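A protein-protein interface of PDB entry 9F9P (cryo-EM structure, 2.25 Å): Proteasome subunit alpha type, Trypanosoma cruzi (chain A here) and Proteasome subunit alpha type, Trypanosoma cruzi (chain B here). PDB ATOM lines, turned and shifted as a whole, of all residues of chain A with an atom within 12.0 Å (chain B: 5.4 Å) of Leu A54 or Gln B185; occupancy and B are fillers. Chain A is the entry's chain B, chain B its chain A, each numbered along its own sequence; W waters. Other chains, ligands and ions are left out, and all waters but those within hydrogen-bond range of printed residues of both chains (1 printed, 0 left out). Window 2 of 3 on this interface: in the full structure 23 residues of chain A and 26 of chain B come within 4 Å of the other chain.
The backbone carbonyl oxygen (O) of Ser B164 is in hydrogen-bond range of the backbone NH (N) of Ala A56. OG1 of Thr A59 lies within hydrogen-bond range of OG of Ser B164. N of His B166 sits at hydrogen-bond distance from O of Leu A54, at 2.8 Å. O of Pro A53 sits close to OE1 of Gln B185 (3.2 Å).
O of Ser A52 lies within hydrogen-bond range of OG1 of Thr A50 (3.3 Å). OG of Ser A52 is in hydrogen-bond range of N of Leu A54 (2.9 Å). OG1 of Thr A59 is in hydrogen-bond range of O of Ala A56 (3.5 Å).
Among the printed residues, pairs that only touch across the chains: Ser A52 with Glu B182 (3.5 Å), Pro A53 with His B166 (3.7 Å), Leu A54 with Tyr B165 (3.5 Å), Leu A54 with Ala B167 (3.4 Å), Leu A54 with Asn B178 (3.7 Å), Leu A54 with Glu B182 (3.9 Å), Leu A54 with Gln B185 (3.8 Å), Ala A55 with Ser B164 (3.9 Å), Ala A55 with Tyr B165 (3.8 Å), Ala A55 with His B166 (3.98 Å) and Ala A56 with His B166 (3.8 Å).
Printed residues of chain B within 4 Å of Ser A52: Glu B182. Of chain B, only Tyr B165, His B166, Ala B167, Asn B178, Glu B182 and Gln B185 come within 4 Å of Leu A54. Printed residues of chain B within 4 Å of Ala A55: Ser B164 (3.9 Å), Tyr B165 (3.8 Å) and His B166 (3.98 Å). Of the printed residues of chain A, His B166 touches Pro A53 (3.7 Å), Leu A54 (2.8 Å), Ala A55 (3.98 Å) and Ala A56 (3.8 Å). Asn B178 touches just one residue of chain A: Leu A54 (3.7 Å). No residue of chain A comes within 4 Å of Leu B181. No residue of chain A comes within 4 Å of Lys B184. Gln B185 touches two residues of chain A. No residue of chain A comes within 4 Å of Lys B186. No residue of chain A comes within 4 Å of Asn B187. No residue of chain A comes within 4 Å of Ala B188. No residue of chain A comes within 4 Å of Pro B189. The nearest printed residue of chain B that does not touch Leu A54 is Phe B190 (4.04 Å). The nearest printed residue of chain A that does not touch Gln B185 is Ala A55 (6.1 Å).
Of the 15 printed residues of chain B, 7 touch a printed residue of chain A. Of the 14 printed residues of chain A, 6 touch a printed residue of chain B. Hydrophobic or aromatic side chains of chain A within 4 Å of the printed part of chain B: Pro A53, Leu A54 and Ala A56.
Water W1 lies within hydrogen-bond range of the backbone carbonyl oxygen (O) of Ala A56 (2.8 Å) and the backbone carbonyl oxygen (O) of Ser B164 (2.9 Å).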
ATOM      1  N   LYS A  48     -18.644   2.027  25.957  1.00  0.00           N
ATOM      2  CA  LYS A  48     -18.949   2.459  24.595  1.00  0.00           C
ATOM      3  C   LYS A  48     -18.982   3.971  24.439  1.00  0.00           C
ATOM      4  O   LYS A  48     -20.038   4.486  24.084  1.00  0.00           O
ATOM      5  CB  LYS A  48     -20.376   2.188  24.106  1.00  0.00           C
ATOM      6  CG  LYS A  48     -21.171   1.137  24.832  1.00  0.00           C
ATOM      7  CD  LYS A  48     -22.556   0.871  24.268  1.00  0.00           C
ATOM      8  CE  LYS A  48     -23.463   2.071  24.189  1.00  0.00           C
ATOM      9  NZ  LYS A  48     -24.679   1.687  23.438  1.00  0.00           N
ATOM     10  N   LYS A  49     -17.865   4.688  24.577  1.00  0.00           N
ATOM     11  CA  LYS A  49     -17.912   6.115  24.273  1.00  0.00           C
ATOM     12  C   LYS A  49     -17.866   6.323  22.754  1.00  0.00           C
ATOM     13  O   LYS A  49     -17.018   5.739  22.081  1.00  0.00           O
ATOM     14  CB  LYS A  49     -16.761   6.880  24.933  1.00  0.00           C
ATOM     15  CG  LYS A  49     -16.420   6.462  26.354  1.00  0.00           C
ATOM     16  CD  LYS A  49     -15.797   7.568  27.187  1.00  0.00           C
ATOM     17  CE  LYS A  49     -14.654   8.282  26.497  1.00  0.00           C
ATOM     18  NZ  LYS A  49     -13.938   9.183  27.430  1.00  0.00           N
ATOM     19  N   THR A  50     -18.761   7.181  22.229  1.00  0.00           N
ATOM     20  CA  THR A  50     -18.686   7.671  20.853  1.00  0.00           C
ATOM     21  C   THR A  50     -17.679   8.826  20.727  1.00  0.00           C
ATOM     22  O   THR A  50     -17.289   9.441  21.721  1.00  0.00           O
ATOM     23  CB  THR A  50     -20.062   8.132  20.331  1.00  0.00           C
ATOM     24  OG1 THR A  50     -20.557   9.160  21.192  1.00  0.00           O
ATOM     25  CG2 THR A  50     -21.086   7.022  20.239  1.00  0.00           C
ATOM     26  N   THR A  51     -17.296   9.142  19.476  1.00  0.00           N
ATOM     27  CA  THR A  51     -16.407  10.265  19.185  1.00  0.00           C
ATOM     28  C   THR A  51     -17.145  11.606  19.303  1.00  0.00           C
ATOM     29  O   THR A  51     -16.513  12.610  19.619  1.00  0.00           O
ATOM     30  CB  THR A  51     -15.748  10.157  17.795  1.00  0.00           C
ATOM     31  OG1 THR A  51     -16.735  10.289  16.767  1.00  0.00           O
ATOM     32  CG2 THR A  51     -14.982   8.864  17.596  1.00  0.00           C
ATOM     33  N   SER A  52     -18.465  11.621  19.043  1.00  0.00           N
ATOM     34  CA  SER A  52     -19.232  12.856  19.013  1.00  0.00           C
ATOM     35  C   SER A  52     -20.707  12.608  19.332  1.00  0.00           C
ATOM     36  O   SER A  52     -21.234  11.533  19.062  1.00  0.00           O
ATOM     37  CB  SER A  52     -19.098  13.515  17.658  1.00  0.00           C
ATOM     38  OG  SER A  52     -20.323  13.523  16.948  1.00  0.00           O
ATOM     39  N   PRO A  53     -21.440  13.613  19.857  1.00  0.00           N
ATOM     40  CA  PRO A  53     -22.883  13.479  20.076  1.00  0.00           C
ATOM     41  C   PRO A  53     -23.776  13.460  18.833  1.00  0.00           C
ATOM     42  O   PRO A  53     -24.997  13.339  18.963  1.00  0.00           O
ATOM     43  CB  PRO A  53     -23.270  14.701  20.916  1.00  0.00           C
ATOM     44  CG  PRO A  53     -22.114  15.685  20.747  1.00  0.00           C
ATOM     45  CD  PRO A  53     -20.897  14.894  20.322  1.00  0.00           C
ATOM     46  N   LEU A  54     -23.168  13.548  17.637  1.00  0.00           N
ATOM     47  CA  LEU A  54     -23.889  13.326  16.395  1.00  0.00           C
ATOM     48  C   LEU A  54     -24.063  11.825  16.147  1.00  0.00           C
ATOM     49  O   LEU A  54     -24.940  11.416  15.375  1.00  0.00           O
ATOM     50  CB  LEU A  54     -23.110  13.976  15.253  1.00  0.00           C
ATOM     51  CG  LEU A  54     -22.962  15.497  15.322  1.00  0.00           C
ATOM     52  CD1 LEU A  54     -21.920  15.964  14.335  1.00  0.00           C
ATOM     53  CD2 LEU A  54     -24.283  16.177  15.064  1.00  0.00           C
ATOM     54  N   ALA A  55     -23.247  10.996  16.812  1.00  0.00           N
ATOM     55  CA  ALA A  55     -23.449   9.555  16.736  1.00  0.00           C
ATOM     56  C   ALA A  55     -24.581   9.124  17.657  1.00  0.00           C
ATOM     57  O   ALA A  55     -24.664   9.588  18.777  1.00  0.00           O
ATOM     58  CB  ALA A  55     -22.188   8.793  17.048  1.00  0.00           C
ATOM     59  N   ALA A  56     -25.428   8.233  17.149  1.00  0.00           N
ATOM     60  CA  ALA A  56     -26.449   7.553  17.924  1.00  0.00           C
ATOM     61  C   ALA A  56     -25.806   6.502  18.829  1.00  0.00           C
ATOM     62  O   ALA A  56     -25.243   5.531  18.331  1.00  0.00           O
ATOM     63  CB  ALA A  56     -27.446   6.930  16.978  1.00  0.00           C
ATOM     64  N   SER A  57     -25.934   6.683  20.156  1.00  0.00           N
ATOM     65  CA  SER A  57     -25.341   5.783  21.146  1.00  0.00           C
ATOM     66  C   SER A  57     -26.006   4.413  21.120  1.00  0.00           C
ATOM     67  O   SER A  57     -25.315   3.402  21.188  1.00  0.00           O
ATOM     68  CB  SER A  57     -25.417   6.367  22.541  1.00  0.00           C
ATOM     69  OG  SER A  57     -24.408   7.347  22.715  1.00  0.00           O
ATOM     70  N   LEU A  58     -27.332   4.387  20.987  1.00  0.00           N
ATOM     71  CA  LEU A  58     -28.103   3.170  21.176  1.00  0.00           C
ATOM     72  C   LEU A  58     -27.614   2.017  20.310  1.00  0.00           C
ATOM     73  O   LEU A  58     -27.576   0.878  20.766  1.00  0.00           O
ATOM     74  CB  LEU A  58     -29.585   3.443  20.902  1.00  0.00           C
ATOM     75  CG  LEU A  58     -30.398   3.857  22.133  1.00  0.00           C
ATOM     76  CD1 LEU A  58     -31.883   4.001  21.790  1.00  0.00           C
ATOM     77  CD2 LEU A  58     -30.203   2.867  23.285  1.00  0.00           C
ATOM     78  N   THR A  59     -27.242   2.301  19.070  1.00  0.00           N
ATOM     79  CA  THR A  59     -26.974   1.248  18.112  1.00  0.00           C
ATOM     80  C   THR A  59     -25.569   0.656  18.276  1.00  0.00           C
ATOM     81  O   THR A  59     -25.308  -0.381  17.687  1.00  0.00           O
ATOM     82  CB  THR A  59     -27.236   1.758  16.678  1.00  0.00           C
ATOM     83  OG1 THR A  59     -26.425   2.898  16.365  1.00  0.00           O
ATOM     84  CG2 THR A  59     -28.697   2.105  16.467  1.00  0.00           C
ATOM     85  N   VAL A  60     -24.671   1.301  19.023  1.00  0.00           N
ATOM     86  CA  VAL A  60     -23.323   0.790  19.218  1.00  0.00           C
ATOM     87  C   VAL A  60     -23.358  -0.425  20.148  1.00  0.00           C
ATOM     88  O   VAL A  60     -23.881  -0.322  21.259  1.00  0.00           O
ATOM     89  CB  VAL A  60     -22.419   1.874  19.828  1.00  0.00           C
ATOM     90  CG1 VAL A  60     -21.018   1.353  20.126  1.00  0.00           C
ATOM     91  CG2 VAL A  60     -22.367   3.130  18.967  1.00  0.00           C
ATOM     92  N   GLU A 204     -25.770   5.244  29.207  1.00  0.00           N
ATOM     93  CA  GLU A 204     -25.793   5.314  27.754  1.00  0.00           C
ATOM     94  C   GLU A 204     -24.416   5.066  27.140  1.00  0.00           C
ATOM     95  O   GLU A 204     -24.351   4.768  25.958  1.00  0.00           O
ATOM     96  CB  GLU A 204     -26.370   6.662  27.315  1.00  0.00           C
ATOM     97  CG  GLU A 204     -27.857   6.788  27.610  1.00  0.00           C
ATOM     98  CD  GLU A 204     -28.414   8.192  27.428  1.00  0.00           C
ATOM     99  OE1 GLU A 204     -28.732   8.840  28.457  1.00  0.00           O
ATOM    100  OE2 GLU A 204     -28.531   8.638  26.260  1.00  0.00           O
ATOM    101  N   SER B 164     -24.531   4.374  13.139  1.00  0.00           N
ATOM    102  CA  SER B 164     -25.723   5.158  12.865  1.00  0.00           C
ATOM    103  C   SER B 164     -25.559   6.545  13.460  1.00  0.00           C
ATOM    104  O   SER B 164     -24.747   6.723  14.341  1.00  0.00           O
ATOM    105  CB  SER B 164     -26.935   4.366  13.303  1.00  0.00           C
ATOM    106  OG  SER B 164     -27.746   5.077  14.198  1.00  0.00           O
ATOM    107  N   TYR B 165     -26.218   7.536  12.859  1.00  0.00           N
ATOM    108  CA  TYR B 165     -26.014   8.946  13.185  1.00  0.00           C
ATOM    109  C   TYR B 165     -27.335   9.706  13.334  1.00  0.00           C
ATOM    110  O   TYR B 165     -28.331   9.318  12.745  1.00  0.00           O
ATOM    111  CB  TYR B 165     -25.178   9.591  12.098  1.00  0.00           C
ATOM    112  CG  TYR B 165     -23.731   9.199  12.170  1.00  0.00           C
ATOM    113  CD1 TYR B 165     -22.856   9.874  13.007  1.00  0.00           C
ATOM    114  CD2 TYR B 165     -23.243   8.118  11.431  1.00  0.00           C
ATOM    115  CE1 TYR B 165     -21.533   9.476  13.134  1.00  0.00           C
ATOM    116  CE2 TYR B 165     -21.923   7.707  11.552  1.00  0.00           C
ATOM    117  CZ  TYR B 165     -21.070   8.401  12.389  1.00  0.00           C
ATOM    118  OH  TYR B 165     -19.751   8.032  12.488  1.00  0.00           O
ATOM    119  N   HIS B 166     -27.338  10.759  14.156  1.00  0.00           N
ATOM    120  CA  HIS B 166     -28.376  11.795  14.113  1.00  0.00           C
ATOM    121  C   HIS B 166     -28.141  12.744  12.928  1.00  0.00           C
ATOM    122  O   HIS B 166     -29.089  13.129  12.262  1.00  0.00           O
ATOM    123  CB  HIS B 166     -28.425  12.591  15.432  1.00  0.00           C
ATOM    124  CG  HIS B 166     -28.785  11.739  16.594  1.00  0.00           C
ATOM    125  ND1 HIS B 166     -27.943  11.563  17.675  1.00  0.00           N
ATOM    126  CD2 HIS B 166     -29.859  10.924  16.781  1.00  0.00           C
ATOM    127  CE1 HIS B 166     -28.508  10.682  18.498  1.00  0.00           C
ATOM    128  NE2 HIS B 166     -29.678  10.283  17.972  1.00  0.00           N
ATOM    129  N   ALA B 167     -26.883  13.136  12.674  1.00  0.00           N
ATOM    130  CA  ALA B 167     -26.529  13.848  11.446  1.00  0.00           C
ATOM    131  C   ALA B 167     -25.041  13.685  11.183  1.00  0.00           C
ATOM    132  O   ALA B 167     -24.315  13.482  12.130  1.00  0.00           O
ATOM    133  CB  ALA B 167     -26.899  15.310  11.609  1.00  0.00           C
ATOM    134  N   ASN B 178     -18.872  19.319  10.770  1.00  0.00           N
ATOM    135  CA  ASN B 178     -19.337  18.572  11.934  1.00  0.00           C
ATOM    136  C   ASN B 178     -19.397  19.485  13.167  1.00  0.00           C
ATOM    137  O   ASN B 178     -20.423  19.503  13.848  1.00  0.00           O
ATOM    138  CB  ASN B 178     -18.556  17.273  12.166  1.00  0.00           C
ATOM    139  CG  ASN B 178     -18.989  16.131  11.249  1.00  0.00           C
ATOM    140  OD1 ASN B 178     -20.169  15.839  11.098  1.00  0.00           O
ATOM    141  ND2 ASN B 178     -18.043  15.461  10.624  1.00  0.00           N
ATOM    142  N   LEU B 181     -22.554  21.443  13.095  1.00  0.00           N
ATOM    143  CA  LEU B 181     -23.793  20.738  13.393  1.00  0.00           C
ATOM    144  C   LEU B 181     -23.873  20.453  14.891  1.00  0.00           C
ATOM    145  O   LEU B 181     -24.978  20.329  15.401  1.00  0.00           O
ATOM    146  CB  LEU B 181     -23.870  19.409  12.627  1.00  0.00           C
ATOM    147  CG  LEU B 181     -23.966  19.448  11.105  1.00  0.00           C
ATOM    148  CD1 LEU B 181     -23.597  18.099  10.518  1.00  0.00           C
ATOM    149  CD2 LEU B 181     -25.353  19.792  10.649  1.00  0.00           C
ATOM    150  N   GLU B 182     -22.715  20.263  15.552  1.00  0.00           N
ATOM    151  CA  GLU B 182     -22.654  20.025  16.994  1.00  0.00           C
ATOM    152  C   GLU B 182     -23.224  21.218  17.752  1.00  0.00           C
ATOM    153  O   GLU B 182     -24.011  21.005  18.669  1.00  0.00           O
ATOM    154  CB  GLU B 182     -21.238  19.752  17.521  1.00  0.00           C
ATOM    155  CG  GLU B 182     -20.758  18.333  17.269  1.00  0.00           C
ATOM    156  CD  GLU B 182     -19.274  18.031  17.460  1.00  0.00           C
ATOM    157  OE1 GLU B 182     -18.821  16.940  16.998  1.00  0.00           O
ATOM    158  OE2 GLU B 182     -18.567  18.872  18.071  1.00  0.00           O
ATOM    159  N   LYS B 183     -22.814  22.443  17.372  1.00  0.00           N
ATOM    160  CA  LYS B 183     -23.350  23.669  17.946  1.00  0.00           C
ATOM    161  C   LYS B 183     -24.867  23.729  17.816  1.00  0.00           C
ATOM    162  O   LYS B 183     -25.568  23.987  18.788  1.00  0.00           O
ATOM    163  CB  LYS B 183     -22.831  24.920  17.240  1.00  0.00           C
ATOM    164  CG  LYS B 183     -21.585  25.548  17.839  1.00  0.00           C
ATOM    165  CD  LYS B 183     -21.407  27.005  17.423  1.00  0.00           C
ATOM    166  CE  LYS B 183     -20.211  27.668  18.080  1.00  0.00           C
ATOM    167  NZ  LYS B 183     -18.936  26.989  17.730  1.00  0.00           N
ATOM    168  N   LYS B 184     -25.366  23.548  16.596  1.00  0.00           N
ATOM    169  CA  LYS B 184     -26.786  23.634  16.335  1.00  0.00           C
ATOM    170  C   LYS B 184     -27.586  22.579  17.106  1.00  0.00           C
ATOM    171  O   LYS B 184     -28.761  22.801  17.378  1.00  0.00           O
ATOM    172  CB  LYS B 184     -27.054  23.497  14.835  1.00  0.00           C
ATOM    173  CG  LYS B 184     -26.765  24.738  14.000  1.00  0.00           C
ATOM    174  CD  LYS B 184     -27.698  25.889  14.289  1.00  0.00           C
ATOM    175  CE  LYS B 184     -27.626  27.003  13.264  1.00  0.00           C
ATOM    176  NZ  LYS B 184     -26.294  27.652  13.240  1.00  0.00           N
ATOM    177  N   GLN B 185     -26.985  21.421  17.401  1.00  0.00           N
ATOM    178  CA  GLN B 185     -27.678  20.314  18.060  1.00  0.00           C
ATOM    179  C   GLN B 185     -28.049  20.697  19.497  1.00  0.00           C
ATOM    180  O   GLN B 185     -29.086  20.264  20.000  1.00  0.00           O
ATOM    181  CB  GLN B 185     -26.804  19.050  18.025  1.00  0.00           C
ATOM    182  CG  GLN B 185     -27.436  17.822  18.677  1.00  0.00           C
ATOM    183  CD  GLN B 185     -26.651  16.547  18.453  1.00  0.00           C
ATOM    184  OE1 GLN B 185     -27.195  15.502  18.098  1.00  0.00           O
ATOM    185  NE2 GLN B 185     -25.348  16.621  18.672  1.00  0.00           N
ATOM    186  N   LYS B 186     -27.182  21.503  20.135  1.00  0.00           N
ATOM    187  CA  LYS B 186     -27.318  21.964  21.512  1.00  0.00           C
ATOM    188  C   LYS B 186     -28.606  22.758  21.751  1.00  0.00           C
ATOM    189  O   LYS B 186     -29.058  22.833  22.891  1.00  0.00           O
ATOM    190  CB  LYS B 186     -26.170  22.907  21.872  1.00  0.00           C
ATOM    191  CG  LYS B 186     -24.774  22.311  21.800  1.00  0.00           C
ATOM    192  CD  LYS B 186     -24.161  22.028  23.160  1.00  0.00           C
ATOM    193  CE  LYS B 186     -22.684  21.700  23.081  1.00  0.00           C
ATOM    194  NZ  LYS B 186     -21.917  22.786  22.421  1.00  0.00           N
ATOM    195  N   ASN B 187     -29.177  23.364  20.702  1.00  0.00           N
ATOM    196  CA  ASN B 187     -30.407  24.141  20.813  1.00  0.00           C
ATOM    197  C   ASN B 187     -31.619  23.227  20.962  1.00  0.00           C
ATOM    198  O   ASN B 187     -32.387  23.368  21.908  1.00  0.00           O
ATOM    199  CB  ASN B 187     -30.667  25.048  19.597  1.00  0.00           C
ATOM    200  CG  ASN B 187     -29.522  25.990  19.280  1.00  0.00           C
ATOM    201  OD1 ASN B 187     -28.554  26.102  20.029  1.00  0.00           O
ATOM    202  ND2 ASN B 187     -29.625  26.674  18.152  1.00  0.00           N
ATOM    203  N   ALA B 188     -31.810  22.336  19.985  1.00  0.00           N
ATOM    204  CA  ALA B 188     -32.917  21.392  19.967  1.00  0.00           C
ATOM    205  C   ALA B 188     -32.450  20.098  19.323  1.00  0.00           C
ATOM    206  O   ALA B 188     -31.879  20.123  18.235  1.00  0.00           O
ATOM    207  CB  ALA B 188     -34.087  21.940  19.183  1.00  0.00           C
ATOM    208  N   PRO B 189     -32.732  18.927  19.928  1.00  0.00           N
ATOM    209  CA  PRO B 189     -32.385  17.655  19.288  1.00  0.00           C
ATOM    210  C   PRO B 189     -33.049  17.512  17.911  1.00  0.00           C
ATOM    211  O   PRO B 189     -34.203  17.870  17.717  1.00  0.00           O
ATOM    212  CB  PRO B 189     -32.859  16.613  20.314  1.00  0.00           C
ATOM    213  CG  PRO B 189     -33.927  17.345  21.110  1.00  0.00           C
ATOM    214  CD  PRO B 189     -33.412  18.762  21.222  1.00  0.00           C
ATOM    215  N   PHE B 190     -32.298  16.948  16.959  1.00  0.00           N
ATOM    216  CA  PHE B 190     -32.715  16.924  15.572  1.00  0.00           C
ATOM    217  C   PHE B 190     -33.990  16.110  15.368  1.00  0.00           C
ATOM    218  O   PHE B 190     -34.712  16.387  14.399  1.00  0.00           O
ATOM    219  CB  PHE B 190     -31.579  16.445  14.680  1.00  0.00           C
ATOM    220  CG  PHE B 190     -30.380  17.356  14.630  1.00  0.00           C
ATOM    221  CD1 PHE B 190     -30.519  18.732  14.702  1.00  0.00           C
ATOM    222  CD2 PHE B 190     -29.104  16.825  14.526  1.00  0.00           C
ATOM    223  CE1 PHE B 190     -29.408  19.560  14.662  1.00  0.00           C
ATOM    224  CE2 PHE B 190     -27.997  17.653  14.473  1.00  0.00           C
ATOM    225  CZ  PHE B 190     -28.154  19.016  14.508  1.00  0.00           C
HETATM  226  O   HOH W   1     -23.439   5.056  16.257  1.00  0.00           O
